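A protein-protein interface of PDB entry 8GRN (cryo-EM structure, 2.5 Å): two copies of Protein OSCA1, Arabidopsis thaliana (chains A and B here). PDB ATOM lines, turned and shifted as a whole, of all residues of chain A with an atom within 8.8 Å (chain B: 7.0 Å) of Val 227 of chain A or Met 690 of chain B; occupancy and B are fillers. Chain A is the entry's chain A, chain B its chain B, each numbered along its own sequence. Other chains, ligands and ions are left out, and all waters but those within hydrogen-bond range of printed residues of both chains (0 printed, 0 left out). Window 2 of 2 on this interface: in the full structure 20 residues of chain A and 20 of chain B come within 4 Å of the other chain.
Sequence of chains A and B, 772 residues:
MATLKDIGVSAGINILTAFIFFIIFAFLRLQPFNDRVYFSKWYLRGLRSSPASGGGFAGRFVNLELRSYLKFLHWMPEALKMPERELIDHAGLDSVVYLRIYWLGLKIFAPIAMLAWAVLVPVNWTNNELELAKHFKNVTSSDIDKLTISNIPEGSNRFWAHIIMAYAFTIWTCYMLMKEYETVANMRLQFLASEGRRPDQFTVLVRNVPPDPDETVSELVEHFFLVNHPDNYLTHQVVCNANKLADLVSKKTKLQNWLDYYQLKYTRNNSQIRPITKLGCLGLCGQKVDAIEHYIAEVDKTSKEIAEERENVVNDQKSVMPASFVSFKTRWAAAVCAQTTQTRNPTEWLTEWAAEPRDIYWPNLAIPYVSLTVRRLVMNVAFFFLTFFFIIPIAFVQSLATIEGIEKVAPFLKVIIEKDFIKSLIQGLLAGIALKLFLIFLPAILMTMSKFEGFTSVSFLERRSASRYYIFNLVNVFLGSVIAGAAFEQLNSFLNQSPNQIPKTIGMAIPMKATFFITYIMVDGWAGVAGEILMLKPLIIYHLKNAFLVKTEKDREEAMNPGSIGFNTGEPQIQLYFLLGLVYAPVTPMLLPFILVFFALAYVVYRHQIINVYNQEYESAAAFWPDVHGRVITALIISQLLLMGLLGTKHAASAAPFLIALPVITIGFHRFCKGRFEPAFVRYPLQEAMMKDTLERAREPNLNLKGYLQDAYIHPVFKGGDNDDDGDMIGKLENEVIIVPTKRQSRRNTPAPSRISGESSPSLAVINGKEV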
ATOM      1  N   LEU A 220      -5.987 -20.856  19.164  1.00  0.00           N
ATOM      2  CA  LEU A 220      -4.671 -20.987  18.783  1.00  0.00           C
ATOM      3  C   LEU A 220      -3.945 -20.904  20.061  1.00  0.00           C
ATOM      4  O   LEU A 220      -2.863 -21.407  20.134  1.00  0.00           O
ATOM      5  CB  LEU A 220      -4.385 -19.793  17.930  1.00  0.00           C
ATOM      6  CG  LEU A 220      -3.377 -19.688  16.799  1.00  0.00           C
ATOM      7  CD1 LEU A 220      -3.827 -20.506  15.619  1.00  0.00           C
ATOM      8  CD2 LEU A 220      -3.296 -18.240  16.372  1.00  0.00           C
ATOM      9  N   VAL A 221      -4.514 -20.315  21.102  1.00  0.00           N
ATOM     10  CA  VAL A 221      -3.915 -20.210  22.407  1.00  0.00           C
ATOM     11  C   VAL A 221      -4.270 -21.451  23.200  1.00  0.00           C
ATOM     12  O   VAL A 221      -3.556 -21.834  24.069  1.00  0.00           O
ATOM     13  CB  VAL A 221      -4.269 -18.884  23.082  1.00  0.00           C
ATOM     14  CG1 VAL A 221      -4.253 -18.975  24.582  1.00  0.00           C
ATOM     15  CG2 VAL A 221      -3.368 -17.780  22.625  1.00  0.00           C
ATOM     16  N   GLU A 222      -5.301 -22.167  22.839  1.00  0.00           N
ATOM     17  CA  GLU A 222      -5.696 -23.318  23.539  1.00  0.00           C
ATOM     18  C   GLU A 222      -4.961 -24.423  23.042  1.00  0.00           C
ATOM     19  O   GLU A 222      -4.502 -25.217  23.783  1.00  0.00           O
ATOM     20  CB  GLU A 222      -7.072 -23.607  23.202  1.00  0.00           C
ATOM     21  CG  GLU A 222      -7.755 -24.507  24.180  1.00  0.00           C
ATOM     22  CD  GLU A 222      -9.231 -24.322  24.117  1.00  0.00           C
ATOM     23  OE1 GLU A 222      -9.731 -24.160  22.989  1.00  0.00           O
ATOM     24  OE2 GLU A 222      -9.876 -24.316  25.180  1.00  0.00           O
ATOM     25  N   HIS A 223      -4.839 -24.547  21.766  1.00  0.00           N
ATOM     26  CA  HIS A 223      -4.035 -25.557  21.169  1.00  0.00           C
ATOM     27  C   HIS A 223      -2.555 -25.465  21.454  1.00  0.00           C
ATOM     28  O   HIS A 223      -1.932 -26.458  21.515  1.00  0.00           O
ATOM     29  CB  HIS A 223      -4.284 -25.516  19.692  1.00  0.00           C
ATOM     30  CG  HIS A 223      -3.768 -26.704  18.948  1.00  0.00           C
ATOM     31  ND1 HIS A 223      -4.363 -27.944  19.014  1.00  0.00           N
ATOM     32  CD2 HIS A 223      -2.717 -26.838  18.104  1.00  0.00           C
ATOM     33  CE1 HIS A 223      -3.696 -28.793  18.256  1.00  0.00           C
ATOM     34  NE2 HIS A 223      -2.691 -28.148  17.692  1.00  0.00           N
ATOM     35  N   PHE A 224      -1.962 -24.322  21.683  1.00  0.00           N
ATOM     36  CA  PHE A 224      -0.590 -24.292  21.991  1.00  0.00           C
ATOM     37  C   PHE A 224      -0.378 -24.751  23.357  1.00  0.00           C
ATOM     38  O   PHE A 224       0.521 -25.486  23.589  1.00  0.00           O
ATOM     39  CB  PHE A 224      -0.018 -22.934  21.813  1.00  0.00           C
ATOM     40  CG  PHE A 224       1.447 -22.809  22.014  1.00  0.00           C
ATOM     41  CD1 PHE A 224       2.304 -22.971  20.972  1.00  0.00           C
ATOM     42  CD2 PHE A 224       1.948 -22.418  23.217  1.00  0.00           C
ATOM     43  CE1 PHE A 224       3.650 -22.815  21.148  1.00  0.00           C
ATOM     44  CE2 PHE A 224       3.284 -22.263  23.405  1.00  0.00           C
ATOM     45  CZ  PHE A 224       4.139 -22.460  22.368  1.00  0.00           C
ATOM     46  N   PHE A 225      -1.184 -24.390  24.319  1.00  0.00           N
ATOM     47  CA  PHE A 225      -0.880 -24.721  25.670  1.00  0.00           C
ATOM     48  C   PHE A 225      -1.415 -26.008  26.093  1.00  0.00           C
ATOM     49  O   PHE A 225      -1.052 -26.475  27.093  1.00  0.00           O
ATOM     50  CB  PHE A 225      -1.298 -23.622  26.601  1.00  0.00           C
ATOM     51  CG  PHE A 225      -0.460 -22.390  26.540  1.00  0.00           C
ATOM     52  CD1 PHE A 225       0.641 -22.262  27.337  1.00  0.00           C
ATOM     53  CD2 PHE A 225      -0.801 -21.345  25.719  1.00  0.00           C
ATOM     54  CE1 PHE A 225       1.415 -21.135  27.291  1.00  0.00           C
ATOM     55  CE2 PHE A 225      -0.032 -20.220  25.662  1.00  0.00           C
ATOM     56  CZ  PHE A 225       1.079 -20.114  26.451  1.00  0.00           C
ATOM     57  N   LEU A 226      -2.255 -26.639  25.339  1.00  0.00           N
ATOM     58  CA  LEU A 226      -2.732 -27.924  25.659  1.00  0.00           C
ATOM     59  C   LEU A 226      -1.851 -28.970  25.100  1.00  0.00           C
ATOM     60  O   LEU A 226      -1.965 -30.086  25.496  1.00  0.00           O
ATOM     61  CB  LEU A 226      -4.121 -28.052  25.107  1.00  0.00           C
ATOM     62  CG  LEU A 226      -5.325 -28.771  25.703  1.00  0.00           C
ATOM     63  CD1 LEU A 226      -5.420 -28.636  27.205  1.00  0.00           C
ATOM     64  CD2 LEU A 226      -6.578 -28.238  25.049  1.00  0.00           C
ATOM     65  N   VAL A 227      -0.968 -28.653  24.171  1.00  0.00           N
ATOM     66  CA  VAL A 227      -0.007 -29.570  23.603  1.00  0.00           C
ATOM     67  C   VAL A 227       1.301 -29.342  24.218  1.00  0.00           C
ATOM     68  O   VAL A 227       1.995 -30.273  24.376  1.00  0.00           O
ATOM     69  CB  VAL A 227       0.134 -29.494  22.077  1.00  0.00           C
ATOM     70  CG1 VAL A 227      -1.186 -29.748  21.402  1.00  0.00           C
ATOM     71  CG2 VAL A 227       0.728 -28.207  21.600  1.00  0.00           C
ATOM     72  N   ASN A 228       1.631 -28.139  24.645  1.00  0.00           N
ATOM     73  CA  ASN A 228       2.942 -27.809  25.149  1.00  0.00           C
ATOM     74  C   ASN A 228       3.109 -27.667  26.621  1.00  0.00           C
ATOM     75  O   ASN A 228       4.201 -27.725  27.055  1.00  0.00           O
ATOM     76  CB  ASN A 228       3.548 -26.637  24.396  1.00  0.00           C
ATOM     77  CG  ASN A 228       3.740 -26.908  22.941  1.00  0.00           C
ATOM     78  OD1 ASN A 228       3.214 -26.211  22.106  1.00  0.00           O
ATOM     79  ND2 ASN A 228       4.505 -27.917  22.630  1.00  0.00           N
ATOM     80  N   HIS A 229       2.068 -27.489  27.409  1.00  0.00           N
ATOM     81  CA  HIS A 229       2.083 -27.403  28.867  1.00  0.00           C
ATOM     82  C   HIS A 229       0.921 -28.212  29.134  1.00  0.00           C
ATOM     83  O   HIS A 229      -0.023 -27.695  29.593  1.00  0.00           O
ATOM     84  CB  HIS A 229       1.815 -26.024  29.338  1.00  0.00           C
ATOM     85  CG  HIS A 229       2.978 -25.111  29.193  1.00  0.00           C
ATOM     86  ND1 HIS A 229       3.892 -24.922  30.197  1.00  0.00           N
ATOM     87  CD2 HIS A 229       3.385 -24.345  28.161  1.00  0.00           C
ATOM     88  CE1 HIS A 229       4.819 -24.082  29.788  1.00  0.00           C
ATOM     89  NE2 HIS A 229       4.532 -23.716  28.555  1.00  0.00           N
ATOM     90  N   PRO A 230       0.986 -29.518  28.902  1.00  0.00           N
ATOM     91  CA  PRO A 230      -0.178 -30.387  28.921  1.00  0.00           C
ATOM     92  C   PRO A 230      -1.017 -30.655  30.168  1.00  0.00           C
ATOM     93  O   PRO A 230      -2.218 -30.635  30.050  1.00  0.00           O
ATOM     94  CB  PRO A 230       0.379 -31.654  28.320  1.00  0.00           C
ATOM     95  CG  PRO A 230       1.817 -31.446  28.035  1.00  0.00           C
ATOM     96  CD  PRO A 230       2.220 -30.302  28.874  1.00  0.00           C
ATOM     97  N   ASP A 231      -0.421 -30.880  31.324  1.00  0.00           N
ATOM     98  CA  ASP A 231      -1.121 -31.193  32.548  1.00  0.00           C
ATOM     99  C   ASP A 231      -1.617 -30.058  33.398  1.00  0.00           C
ATOM    100  O   ASP A 231      -2.614 -30.209  34.056  1.00  0.00           O
ATOM    101  CB  ASP A 231      -0.228 -32.061  33.392  1.00  0.00           C
ATOM    102  CG  ASP A 231       0.805 -32.774  32.587  1.00  0.00           C
ATOM    103  OD1 ASP A 231       0.509 -33.880  32.092  1.00  0.00           O
ATOM    104  OD2 ASP A 231       1.921 -32.236  32.451  1.00  0.00           O
ATOM    105  N   TYR A 233      -2.957 -26.554  32.758  1.00  0.00           N
ATOM    106  CA  TYR A 233      -3.317 -25.464  31.935  1.00  0.00           C
ATOM    107  C   TYR A 233      -4.711 -25.542  32.356  1.00  0.00           C
ATOM    108  O   TYR A 233      -5.197 -26.613  32.488  1.00  0.00           O
ATOM    109  CB  TYR A 233      -3.166 -25.743  30.467  1.00  0.00           C
ATOM    110  CG  TYR A 233      -4.096 -24.984  29.561  1.00  0.00           C
ATOM    111  CD1 TYR A 233      -3.873 -23.667  29.248  1.00  0.00           C
ATOM    112  CD2 TYR A 233      -5.203 -25.595  29.022  1.00  0.00           C
ATOM    113  CE1 TYR A 233      -4.736 -22.982  28.431  1.00  0.00           C
ATOM    114  CE2 TYR A 233      -6.066 -24.915  28.214  1.00  0.00           C
ATOM    115  CZ  TYR A 233      -5.821 -23.617  27.926  1.00  0.00           C
ATOM    116  OH  TYR A 233      -6.692 -22.966  27.122  1.00  0.00           O
ATOM    117  N   GLN A 342       9.511 -20.556  24.679  1.00  0.00           N
ATOM    118  CA  GLN A 342       8.530 -21.420  24.178  1.00  0.00           C
ATOM    119  C   GLN A 342       8.587 -21.813  22.778  1.00  0.00           C
ATOM    120  O   GLN A 342       8.091 -22.838  22.452  1.00  0.00           O
ATOM    121  CB  GLN A 342       7.184 -20.802  24.480  1.00  0.00           C
ATOM    122  CG  GLN A 342       7.024 -20.120  25.809  1.00  0.00           C
ATOM    123  CD  GLN A 342       6.554 -21.068  26.862  1.00  0.00           C
ATOM    124  OE1 GLN A 342       5.791 -21.961  26.586  1.00  0.00           O
ATOM    125  NE2 GLN A 342       7.022 -20.890  28.067  1.00  0.00           N
ATOM    126  N   THR B 330      11.589 -37.068  30.259  1.00  0.00           N
ATOM    127  CA  THR B 330      11.297 -36.380  29.078  1.00  0.00           C
ATOM    128  C   THR B 330      12.355 -35.364  28.862  1.00  0.00           C
ATOM    129  O   THR B 330      13.096 -35.102  29.723  1.00  0.00           O
ATOM    130  CB  THR B 330       9.942 -35.727  29.177  1.00  0.00           C
ATOM    131  OG1 THR B 330       9.752 -35.172  30.464  1.00  0.00           O
ATOM    132  CG2 THR B 330       8.843 -36.691  28.919  1.00  0.00           C
ATOM    133  N   ARG B 331      12.429 -34.778  27.693  1.00  0.00           N
ATOM    134  CA  ARG B 331      13.360 -33.763  27.333  1.00  0.00           C
ATOM    135  C   ARG B 331      12.766 -32.449  27.556  1.00  0.00           C
ATOM    136  O   ARG B 331      13.452 -31.512  27.428  1.00  0.00           O
ATOM    137  CB  ARG B 331      13.581 -33.846  25.848  1.00  0.00           C
ATOM    138  CG  ARG B 331      14.644 -34.746  25.318  1.00  0.00           C
ATOM    139  CD  ARG B 331      14.542 -34.792  23.820  1.00  0.00           C
ATOM    140  NE  ARG B 331      13.699 -35.893  23.446  1.00  0.00           N
ATOM    141  CZ  ARG B 331      14.123 -36.973  22.825  1.00  0.00           C
ATOM    142  NH1 ARG B 331      15.376 -37.090  22.488  1.00  0.00           N
ATOM    143  NH2 ARG B 331      13.289 -37.933  22.534  1.00  0.00           N
ATOM    144  N   TRP B 332      11.486 -32.337  27.828  1.00  0.00           N
ATOM    145  CA  TRP B 332      10.821 -31.139  28.137  1.00  0.00           C
ATOM    146  C   TRP B 332      11.032 -30.866  29.537  1.00  0.00           C
ATOM    147  O   TRP B 332      11.144 -29.735  29.849  1.00  0.00           O
ATOM    148  CB  TRP B 332       9.364 -31.377  27.900  1.00  0.00           C
ATOM    149  CG  TRP B 332       8.399 -30.258  28.178  1.00  0.00           C
ATOM    150  CD1 TRP B 332       7.884 -29.400  27.277  1.00  0.00           C
ATOM    151  CD2 TRP B 332       7.782 -29.933  29.427  1.00  0.00           C
ATOM    152  NE1 TRP B 332       7.025 -28.537  27.877  1.00  0.00           N
ATOM    153  CE2 TRP B 332       6.949 -28.843  29.204  1.00  0.00           C
ATOM    154  CE3 TRP B 332       7.876 -30.448  30.721  1.00  0.00           C
ATOM    155  CZ2 TRP B 332       6.220 -28.259  30.209  1.00  0.00           C
ATOM    156  CZ3 TRP B 332       7.166 -29.862  31.711  1.00  0.00           C
ATOM    157  CH2 TRP B 332       6.342 -28.784  31.456  1.00  0.00           C
ATOM    158  N   TYR B 684      16.954 -23.692  24.718  1.00  0.00           N
ATOM    159  CA  TYR B 684      16.183 -24.717  24.021  1.00  0.00           C
ATOM    160  C   TYR B 684      14.740 -24.521  24.166  1.00  0.00           C
ATOM    161  O   TYR B 684      14.229 -24.675  25.228  1.00  0.00           O
ATOM    162  CB  TYR B 684      16.492 -26.089  24.554  1.00  0.00           C
ATOM    163  CG  TYR B 684      16.151 -27.230  23.620  1.00  0.00           C
ATOM    164  CD1 TYR B 684      16.331 -27.117  22.264  1.00  0.00           C
ATOM    165  CD2 TYR B 684      15.646 -28.413  24.099  1.00  0.00           C
ATOM    166  CE1 TYR B 684      16.011 -28.144  21.411  1.00  0.00           C
ATOM    167  CE2 TYR B 684      15.331 -29.447  23.252  1.00  0.00           C
ATOM    168  CZ  TYR B 684      15.520 -29.302  21.908  1.00  0.00           C
ATOM    169  OH  TYR B 684      15.219 -30.322  21.047  1.00  0.00           O
ATOM    170  N   PRO B 685      14.049 -24.203  23.097  1.00  0.00           N
ATOM    171  CA  PRO B 685      12.657 -23.957  23.138  1.00  0.00           C
ATOM    172  C   PRO B 685      11.889 -25.135  23.686  1.00  0.00           C
ATOM    173  O   PRO B 685      12.375 -26.181  23.599  1.00  0.00           O
ATOM    174  CB  PRO B 685      12.394 -23.647  21.716  1.00  0.00           C
ATOM    175  CG  PRO B 685      13.535 -24.055  20.906  1.00  0.00           C
ATOM    176  CD  PRO B 685      14.644 -23.840  21.815  1.00  0.00           C
ATOM    177  N   LEU B 686      10.708 -24.998  24.236  1.00  0.00           N
ATOM    178  CA  LEU B 686       9.940 -26.062  24.845  1.00  0.00           C
ATOM    179  C   LEU B 686       8.984 -26.666  23.915  1.00  0.00           C
ATOM    180  O   LEU B 686       8.436 -27.673  24.217  1.00  0.00           O
ATOM    181  CB  LEU B 686       9.224 -25.554  26.099  1.00  0.00           C
ATOM    182  CG  LEU B 686       9.629 -25.866  27.530  1.00  0.00           C
ATOM    183  CD1 LEU B 686      11.105 -25.695  27.769  1.00  0.00           C
ATOM    184  CD2 LEU B 686       8.848 -24.958  28.439  1.00  0.00           C
ATOM    185  N   GLN B 687       8.766 -26.084  22.759  1.00  0.00           N
ATOM    186  CA  GLN B 687       7.951 -26.663  21.754  1.00  0.00           C
ATOM    187  C   GLN B 687       8.742 -27.555  20.960  1.00  0.00           C
ATOM    188  O   GLN B 687       8.207 -28.407  20.355  1.00  0.00           O
ATOM    189  CB  GLN B 687       7.473 -25.626  20.830  1.00  0.00           C
ATOM    190  CG  GLN B 687       6.390 -26.032  19.867  1.00  0.00           C
ATOM    191  CD  GLN B 687       6.214 -25.042  18.757  1.00  0.00           C
ATOM    192  OE1 GLN B 687       5.111 -24.788  18.317  1.00  0.00           O
ATOM    193  NE2 GLN B 687       7.304 -24.476  18.299  1.00  0.00           N
ATOM    194  N   GLU B 688      10.039 -27.422  20.950  1.00  0.00           N
ATOM    195  CA  GLU B 688      10.930 -28.250  20.225  1.00  0.00           C
ATOM    196  C   GLU B 688      11.195 -29.512  20.945  1.00  0.00           C
ATOM    197  O   GLU B 688      11.274 -30.519  20.330  1.00  0.00           O
ATOM    198  CB  GLU B 688      12.138 -27.428  20.104  1.00  0.00           C
ATOM    199  CG  GLU B 688      12.717 -27.266  18.724  1.00  0.00           C
ATOM    200  CD  GLU B 688      11.898 -26.357  17.862  1.00  0.00           C
ATOM    201  OE1 GLU B 688      11.323 -25.406  18.405  1.00  0.00           O
ATOM    202  OE2 GLU B 688      11.825 -26.603  16.647  1.00  0.00           O
ATOM    203  N   ALA B 689      11.261 -29.507  22.254  1.00  0.00           N
ATOM    204  CA  ALA B 689      11.425 -30.642  23.092  1.00  0.00           C
ATOM    205  C   ALA B 689      10.221 -31.456  23.208  1.00  0.00           C
ATOM    206  O   ALA B 689      10.344 -32.616  23.400  1.00  0.00           O
ATOM    207  CB  ALA B 689      11.737 -30.108  24.383  1.00  0.00           C
ATOM    208  N   MET B 690       9.030 -30.912  23.117  1.00  0.00           N
ATOM    209  CA  MET B 690       7.830 -31.680  23.052  1.00  0.00           C
ATOM    210  C   MET B 690       7.581 -32.325  21.726  1.00  0.00           C
ATOM    211  O   MET B 690       7.047 -33.373  21.699  1.00  0.00           O
ATOM    212  CB  MET B 690       6.649 -30.871  23.486  1.00  0.00           C
ATOM    213  CG  MET B 690       5.379 -31.663  23.683  1.00  0.00           C
ATOM    214  SD  MET B 690       4.906 -31.799  25.394  1.00  0.00           S
ATOM    215  CE  MET B 690       5.896 -33.184  25.926  1.00  0.00           C
ATOM    216  N   MET B 691       7.962 -31.774  20.606  1.00  0.00           N
ATOM    217  CA  MET B 691       7.823 -32.430  19.352  1.00  0.00           C
ATOM    218  C   MET B 691       8.754 -33.551  19.117  1.00  0.00           C
ATOM    219  O   MET B 691       8.411 -34.410  18.377  1.00  0.00           O
ATOM    220  CB  MET B 691       8.107 -31.500  18.250  1.00  0.00           C
ATOM    221  CG  MET B 691       7.173 -30.350  18.006  1.00  0.00           C
ATOM    222  SD  MET B 691       7.568 -29.657  16.390  1.00  0.00           S
ATOM    223  CE  MET B 691       8.351 -28.111  16.811  1.00  0.00           C
ATOM    224  N   LYS B 692       9.934 -33.590  19.714  1.00  0.00           N
ATOM    225  CA  LYS B 692      10.895 -34.612  19.550  1.00  0.00           C
ATOM    226  C   LYS B 692      10.506 -35.699  20.392  1.00  0.00           C
ATOM    227  O   LYS B 692      10.725 -36.810  20.053  1.00  0.00           O
ATOM    228  CB  LYS B 692      12.208 -34.082  19.998  1.00  0.00           C
ATOM    229  CG  LYS B 692      13.407 -34.618  19.259  1.00  0.00           C
ATOM    230  CD  LYS B 692      14.662 -33.978  19.794  1.00  0.00           C
ATOM    231  CE  LYS B 692      15.913 -34.618  19.234  1.00  0.00           C
ATOM    232  NZ  LYS B 692      15.593 -35.860  18.511  1.00  0.00           N
ATOM    233  N   ASP B 693       9.822 -35.425  21.453  1.00  0.00           N
ATOM    234  CA  ASP B 693       9.451 -36.389  22.412  1.00  0.00           C
ATOM    235  C   ASP B 693       8.207 -37.086  22.120  1.00  0.00           C
ATOM    236  O   ASP B 693       8.000 -38.144  22.618  1.00  0.00           O
ATOM    237  CB  ASP B 693       9.257 -35.652  23.685  1.00  0.00           C
ATOM    238  CG  ASP B 693      10.288 -35.926  24.700  1.00  0.00           C
ATOM    239  OD1 ASP B 693      10.984 -36.949  24.633  1.00  0.00           O
ATOM    240  OD2 ASP B 693      10.367 -35.101  25.608  1.00  0.00           O
ATOM    241  N   THR B 694       7.341 -36.511  21.327  1.00  0.00           N
ATOM    242  CA  THR B 694       6.110 -37.130  20.931  1.00  0.00           C
ATOM    243  C   THR B 694       6.189 -37.838  19.668  1.00  0.00           C
ATOM    244  O   THR B 694       5.264 -38.500  19.322  1.00  0.00           O
ATOM    245  CB  THR B 694       4.990 -36.154  20.729  1.00  0.00           C
ATOM    246  OG1 THR B 694       5.362 -35.208  19.741  1.00  0.00           O
ATOM    247  CG2 THR B 694       4.658 -35.455  22.008  1.00  0.00           C
ATOM    248  N   LEU B 695       7.266 -37.718  18.946  1.00  0.00           N
ATOM    249  CA  LEU B 695       7.469 -38.439  17.734  1.00  0.00           C
ATOM    250  C   LEU B 695       8.316 -39.636  17.970  1.00  0.00           C
ATOM    251  O   LEU B 695       8.451 -40.419  17.087  1.00  0.00           O
ATOM    252  CB  LEU B 695       8.171 -37.542  16.754  1.00  0.00           C
ATOM    253  CG  LEU B 695       7.415 -36.737  15.723  1.00  0.00           C
ATOM    254  CD1 LEU B 695       8.283 -35.569  15.310  1.00  0.00           C
ATOM    255  CD2 LEU B 695       7.157 -37.637  14.535  1.00  0.00           C
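No position is printed for both chains.
Among the printed residues, pairs that only touch across the chains: Phe 224 of chain A with Gln 687 of chain B (3.7 Å), Asn 228 of chain A with Gln 687 of chain B (3.8 Å), Asn 228 of chain A with Met 690 of chain B (3.7 Å) and Gln 342 of chain A with Leu 686 of chain B (3.8 Å).
The side-chain hydroxyl (OG1) of Thr 694 of chain B sits at hydrogen-bond distance from the backbone carbonyl oxygen (O) of Met 690 of chain B (3.2 Å). O of Phe 224 of chain A sits close to OD1 of Asn 228 of chain A, at 3.2 Å. A ring nitrogen (NE2) of His 229 of chain A sits at hydrogen-bond distance from the side-chain amide oxygen (OE1) of Gln 342 of chain A (2.9 Å).
Of the printed residues of chain B, Phe 224 of chain A touches Gln 687. Of chain B, only Met 690 comes within 4 Å of Val 227 of chain A. Printed residues of chain B within 4 Å of Gln 342 of chain A: Leu 686 and Gln 687. Of the printed residues of chain A, Trp 332 of chain B touches Asn 228. Of the printed residues of chain A, Gln 687 of chain B touches Phe 224, Asn 228 and Gln 342. No residue of chain A comes within 4 Å of Ala 689 of chain B. Of chain A, only Val 227 (3.4 Å) and Asn 228 (3.7 Å) come within 4 Å of Met 690 of chain B. The nearest printed residue of chain A that does not touch Leu 686 of chain B is Asn 228 of chain A (4.2 Å).
Of the 14 printed residues of chain A, 4 touch a printed residue of chain B. Hydrophobic or aromatic side chains of chain A within 4 Å of the printed part of chain B: Phe 224. Along chain A the printed residues that touch a printed residue of chain B span positions 224 to 342. Of the 15 printed residues of chain B, 4 touch a printed residue of chain A. Among the printed residues, 7 pairs touch across the chains. Among the printed residues, no Asp or Glu carboxylate lies within 4 Å of a Lys or Arg side-chain nitrogen of the other chain.
SD of Met 690 of chain B sits close to O of Val 227 of chain A, at 3.4 Å. The backbone carbonyl oxygen (O) of Gln 342 of chain A sits close to the backbone NH (N) of Gln 687 of chain B (3.3 Å). The indole nitrogen (NE1) of Trp 332 of chain B is in hydrogen-bond range of the backbone carbonyl oxygen (O) of Asn 228 of chain A.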
